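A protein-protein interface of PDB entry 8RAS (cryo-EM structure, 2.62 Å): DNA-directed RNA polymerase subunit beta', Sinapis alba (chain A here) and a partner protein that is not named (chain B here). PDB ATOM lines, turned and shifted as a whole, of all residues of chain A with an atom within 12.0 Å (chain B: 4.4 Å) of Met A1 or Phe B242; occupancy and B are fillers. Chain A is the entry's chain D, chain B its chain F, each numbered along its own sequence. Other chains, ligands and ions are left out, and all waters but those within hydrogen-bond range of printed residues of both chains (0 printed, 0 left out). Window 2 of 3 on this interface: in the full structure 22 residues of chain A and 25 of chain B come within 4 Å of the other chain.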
ATOM      1  N   MET A   1      -4.766 -17.696  23.412  1.00  0.00           N
ATOM      2  CA  MET A   1      -5.322 -18.798  22.633  1.00  0.00           C
ATOM      3  C   MET A   1      -5.111 -20.155  23.284  1.00  0.00           C
ATOM      4  O   MET A   1      -3.979 -20.589  23.493  1.00  0.00           O
ATOM      5  CB  MET A   1      -4.724 -18.811  21.226  1.00  0.00           C
ATOM      6  CG  MET A   1      -5.509 -18.015  20.197  1.00  0.00           C
ATOM      7  SD  MET A   1      -7.285 -18.041  20.509  1.00  0.00           S
ATOM      8  CE  MET A   1      -7.541 -16.412  21.198  1.00  0.00           C
ATOM      9  N   ILE A   2      -6.213 -20.822  23.598  1.00  0.00           N
ATOM     10  CA  ILE A   2      -6.182 -22.190  24.097  1.00  0.00           C
ATOM     11  C   ILE A   2      -6.284 -23.122  22.900  1.00  0.00           C
ATOM     12  O   ILE A   2      -7.233 -23.033  22.115  1.00  0.00           O
ATOM     13  CB  ILE A   2      -7.323 -22.446  25.091  1.00  0.00           C
ATOM     14  CG1 ILE A   2      -7.173 -21.561  26.326  1.00  0.00           C
ATOM     15  CG2 ILE A   2      -7.358 -23.908  25.486  1.00  0.00           C
ATOM     16  CD1 ILE A   2      -8.346 -21.660  27.267  1.00  0.00           C
ATOM     17  N   ASP A   3      -5.308 -24.012  22.756  1.00  0.00           N
ATOM     18  CA  ASP A   3      -5.286 -24.912  21.613  1.00  0.00           C
ATOM     19  C   ASP A   3      -6.471 -25.868  21.655  1.00  0.00           C
ATOM     20  O   ASP A   3      -6.869 -26.346  22.720  1.00  0.00           O
ATOM     21  CB  ASP A   3      -3.976 -25.697  21.581  1.00  0.00           C
ATOM     22  CG  ASP A   3      -2.787 -24.825  21.239  1.00  0.00           C
ATOM     23  OD1 ASP A   3      -2.996 -23.713  20.709  1.00  0.00           O
ATOM     24  OD2 ASP A   3      -1.642 -25.250  21.497  1.00  0.00           O
ATOM     25  N   ARG A   4      -7.041 -26.138  20.484  1.00  0.00           N
ATOM     26  CA  ARG A   4      -8.134 -27.099  20.363  1.00  0.00           C
ATOM     27  C   ARG A   4      -7.532 -28.490  20.496  1.00  0.00           C
ATOM     28  O   ARG A   4      -7.127 -29.116  19.516  1.00  0.00           O
ATOM     29  CB  ARG A   4      -8.873 -26.923  19.044  1.00  0.00           C
ATOM     30  CG  ARG A   4      -9.601 -25.599  18.925  1.00  0.00           C
ATOM     31  CD  ARG A   4     -10.902 -25.615  19.702  1.00  0.00           C
ATOM     32  NE  ARG A   4     -11.406 -24.269  19.944  1.00  0.00           N
ATOM     33  CZ  ARG A   4     -12.669 -23.982  20.225  1.00  0.00           C
ATOM     34  NH1 ARG A   4     -13.591 -24.927  20.307  1.00  0.00           N
ATOM     35  NH2 ARG A   4     -13.017 -22.715  20.428  1.00  0.00           N
ATOM     36  N   TYR A   5      -7.469 -28.970  21.734  1.00  0.00           N
ATOM     37  CA  TYR A   5      -6.779 -30.217  22.029  1.00  0.00           C
ATOM     38  C   TYR A   5      -7.477 -31.400  21.371  1.00  0.00           C
ATOM     39  O   TYR A   5      -8.705 -31.512  21.390  1.00  0.00           O
ATOM     40  CB  TYR A   5      -6.705 -30.428  23.539  1.00  0.00           C
ATOM     41  CG  TYR A   5      -6.133 -29.250  24.292  1.00  0.00           C
ATOM     42  CD1 TYR A   5      -4.831 -28.828  24.073  1.00  0.00           C
ATOM     43  CD2 TYR A   5      -6.897 -28.559  25.221  1.00  0.00           C
ATOM     44  CE1 TYR A   5      -4.305 -27.751  24.757  1.00  0.00           C
ATOM     45  CE2 TYR A   5      -6.379 -27.482  25.909  1.00  0.00           C
ATOM     46  CZ  TYR A   5      -5.084 -27.082  25.673  1.00  0.00           C
ATOM     47  OH  TYR A   5      -4.562 -26.008  26.357  1.00  0.00           O
ATOM     48  N   MET B 236     -14.893 -17.681  26.788  1.00  0.00           N
ATOM     49  CA  MET B 236     -14.259 -16.454  27.256  1.00  0.00           C
ATOM     50  C   MET B 236     -13.191 -15.981  26.282  1.00  0.00           C
ATOM     51  O   MET B 236     -13.083 -14.779  26.007  1.00  0.00           O
ATOM     52  CB  MET B 236     -13.667 -16.677  28.647  1.00  0.00           C
ATOM     53  CG  MET B 236     -12.491 -15.788  28.984  1.00  0.00           C
ATOM     54  SD  MET B 236     -11.716 -16.239  30.546  1.00  0.00           S
ATOM     55  CE  MET B 236     -10.081 -16.695  29.984  1.00  0.00           C
ATOM     56  N   GLU B 237     -12.394 -16.907  25.747  1.00  0.00           N
ATOM     57  CA  GLU B 237     -11.402 -16.525  24.750  1.00  0.00           C
ATOM     58  C   GLU B 237     -12.057 -16.084  23.448  1.00  0.00           C
ATOM     59  O   GLU B 237     -11.514 -15.227  22.743  1.00  0.00           O
ATOM     60  CB  GLU B 237     -10.434 -17.677  24.502  1.00  0.00           C
ATOM     61  CG  GLU B 237      -9.459 -17.902  25.639  1.00  0.00           C
ATOM     62  CD  GLU B 237      -8.119 -18.401  25.156  1.00  0.00           C
ATOM     63  OE1 GLU B 237      -8.097 -19.202  24.199  1.00  0.00           O
ATOM     64  OE2 GLU B 237      -7.087 -17.987  25.724  1.00  0.00           O
ATOM     65  N   GLY B 240     -13.059 -12.424  23.657  1.00  0.00           N
ATOM     66  CA  GLY B 240     -11.973 -11.461  23.600  1.00  0.00           C
ATOM     67  C   GLY B 240     -11.055 -11.444  24.805  1.00  0.00           C
ATOM     68  O   GLY B 240     -10.089 -10.667  24.804  1.00  0.00           O
ATOM     69  N   ARG B 241     -11.285 -12.250  25.838  1.00  0.00           N
ATOM     70  CA  ARG B 241     -10.406 -12.305  27.002  1.00  0.00           C
ATOM     71  C   ARG B 241      -9.591 -13.590  26.929  1.00  0.00           C
ATOM     72  O   ARG B 241     -10.134 -14.687  27.089  1.00  0.00           O
ATOM     73  CB  ARG B 241     -11.195 -12.231  28.307  1.00  0.00           C
ATOM     74  CG  ARG B 241     -10.314 -12.341  29.543  1.00  0.00           C
ATOM     75  CD  ARG B 241     -11.069 -11.993  30.809  1.00  0.00           C
ATOM     76  NE  ARG B 241     -10.213 -12.042  31.988  1.00  0.00           N
ATOM     77  CZ  ARG B 241     -10.349 -12.915  32.975  1.00  0.00           C
ATOM     78  NH1 ARG B 241     -11.302 -13.833  32.959  1.00  0.00           N
ATOM     79  NH2 ARG B 241      -9.512 -12.865  34.007  1.00  0.00           N
ATOM     80  N   PHE B 242      -8.292 -13.445  26.699  1.00  0.00           N
ATOM     81  CA  PHE B 242      -7.400 -14.584  26.555  1.00  0.00           C
ATOM     82  C   PHE B 242      -7.094 -15.220  27.904  1.00  0.00           C
ATOM     83  O   PHE B 242      -7.072 -14.556  28.943  1.00  0.00           O
ATOM     84  CB  PHE B 242      -6.104 -14.153  25.873  1.00  0.00           C
ATOM     85  CG  PHE B 242      -6.316 -13.510  24.536  1.00  0.00           C
ATOM     86  CD1 PHE B 242      -7.417 -13.840  23.768  1.00  0.00           C
ATOM     87  CD2 PHE B 242      -5.440 -12.551  24.062  1.00  0.00           C
ATOM     88  CE1 PHE B 242      -7.629 -13.248  22.546  1.00  0.00           C
ATOM     89  CE2 PHE B 242      -5.647 -11.957  22.835  1.00  0.00           C
ATOM     90  CZ  PHE B 242      -6.742 -12.312  22.075  1.00  0.00           C
ATOM     91  N   ALA B 243      -6.861 -16.529  27.875  1.00  0.00           N
ATOM     92  CA  ALA B 243      -6.560 -17.260  29.094  1.00  0.00           C
ATOM     93  C   ALA B 243      -5.147 -16.952  29.569  1.00  0.00           C
ATOM     94  O   ALA B 243      -4.216 -16.825  28.769  1.00  0.00           O
ATOM     95  CB  ALA B 243      -6.727 -18.763  28.870  1.00  0.00           C
ATOM     96  N   THR B 244      -4.995 -16.827  30.880  1.00  0.00           N
ATOM     97  CA  THR B 244      -3.717 -16.579  31.520  1.00  0.00           C
ATOM     98  C   THR B 244      -3.282 -17.827  32.284  1.00  0.00           C
ATOM     99  O   THR B 244      -3.920 -18.882  32.209  1.00  0.00           O
ATOM    100  CB  THR B 244      -3.812 -15.356  32.435  1.00  0.00           C
ATOM    101  OG1 THR B 244      -4.840 -15.565  33.410  1.00  0.00           O
ATOM    102  CG2 THR B 244      -4.135 -14.111  31.626  1.00  0.00           C
ATOM    103  N   ASN B 270       0.997 -25.913  25.356  1.00  0.00           N
ATOM    104  CA  ASN B 270       0.255 -24.707  25.008  1.00  0.00           C
ATOM    105  C   ASN B 270       0.738 -23.515  25.824  1.00  0.00           C
ATOM    106  O   ASN B 270       0.915 -22.415  25.287  1.00  0.00           O
ATOM    107  CB  ASN B 270      -1.239 -24.937  25.228  1.00  0.00           C
ATOM    108  CG  ASN B 270      -2.090 -23.793  24.721  1.00  0.00           C
ATOM    109  OD1 ASN B 270      -1.593 -22.853  24.103  1.00  0.00           O
ATOM    110  ND2 ASN B 270      -3.385 -23.865  24.990  1.00  0.00           N
ATOM    111  N   PHE B 277       1.721 -13.902  29.285  1.00  0.00           N
ATOM    112  CA  PHE B 277       0.740 -14.104  30.342  1.00  0.00           C
ATOM    113  C   PHE B 277       0.270 -15.547  30.451  1.00  0.00           C
ATOM    114  O   PHE B 277      -0.429 -15.880  31.413  1.00  0.00           O
ATOM    115  CB  PHE B 277      -0.465 -13.178  30.138  1.00  0.00           C
ATOM    116  CG  PHE B 277      -1.075 -13.257  28.768  1.00  0.00           C
ATOM    117  CD1 PHE B 277      -0.615 -12.448  27.742  1.00  0.00           C
ATOM    118  CD2 PHE B 277      -2.115 -14.129  28.507  1.00  0.00           C
ATOM    119  CE1 PHE B 277      -1.177 -12.514  26.486  1.00  0.00           C
ATOM    120  CE2 PHE B 277      -2.678 -14.201  27.251  1.00  0.00           C
ATOM    121  CZ  PHE B 277      -2.208 -13.393  26.240  1.00  0.00           C
ATOM    122  N   MET B 278       0.632 -16.405  29.500  1.00  0.00           N
ATOM    123  CA  MET B 278       0.310 -17.824  29.564  1.00  0.00           C
ATOM    124  C   MET B 278       1.481 -18.677  30.028  1.00  0.00           C
ATOM    125  O   MET B 278       1.356 -19.902  30.065  1.00  0.00           O
ATOM    126  CB  MET B 278      -0.168 -18.321  28.197  1.00  0.00           C
ATOM    127  CG  MET B 278      -1.195 -17.427  27.532  1.00  0.00           C
ATOM    128  SD  MET B 278      -1.465 -17.834  25.797  1.00  0.00           S
ATOM    129  CE  MET B 278      -0.803 -19.494  25.727  1.00  0.00           C
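Hydrophobic or aromatic side chains of chain A within 4 Å of the printed part of chain B: Met A1, Ile A2 and Tyr A5.
Among the printed residues, no Asp or Glu carboxylate lies within 4 Å of a Lys or Arg side-chain nitrogen of the other chain.
Among the printed residues, merely in contact across the chains: Ile A2 with Asn B270 (3.4 Å), Met A1 with Phe B242 (3.4 Å) and Ile A2 with Ala B243 (3.7 Å).
The backbone NH (N) of Ala B243 lies within hydrogen-bond range of the side-chain carboxylate (OE2) of Glu B237, at 2.6 Å.
The backbone NH (N) of Met A1 lies within hydrogen-bond range of the side-chain carboxylate (OE2) of Glu B237 (3.3 Å).
The backbone carbonyl oxygen (O) of Met A1 sits close to the side-chain amide oxygen (OD1) of Asn B270 (3.3 Å).
The backbone NH (N) of Ile A2 is in hydrogen-bond range of the side-chain carboxylate (OE1) of Glu B237, at 2.6 Å.
The backbone NH (N) of Asp A3 lies close to the side-chain amide nitrogen (ND2) of Asn B270 (3.0 Å).
The side-chain hydroxyl (OH) of Tyr A5 sits at hydrogen-bond distance from the side-chain amide nitrogen (ND2) of Asn B270 (2.8 Å).
Of the printed residues of chain B, Met A1 touches Glu B237 (3.2 Å), Phe B242 (3.4 Å) and Asn B270 (3.3 Å).
Printed residues of chain B within 4 Å of Ile A2: Glu B237, Ala B243 and Asn B270.
Of the printed residues of chain B, Asp A3 touches Asn B270.
Of the printed residues of chain B, Tyr A5 touches Asn B270 (2.8 Å).
Met B236 touches none of the printed residues of chain A.
Glu B237 touches two residues of chain A.
No residue of chain A comes within 4 Å of Gly B240.
No residue of chain A comes within 4 Å of Arg B241.
Of chain A, only Met A1 (3.4 Å) comes within 4 Å of Phe B242.
Of the printed residues of chain A, Ala B243 touches Ile A2.
No residue of chain A comes within 4 Å of Thr B244.
The nearest residue of chain A that does not touch Phe B242 is Ile A2 (6.5 Å).
The nearest printed residue of chain B that does not touch Tyr A5 is Met B278 (7.5 Å).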
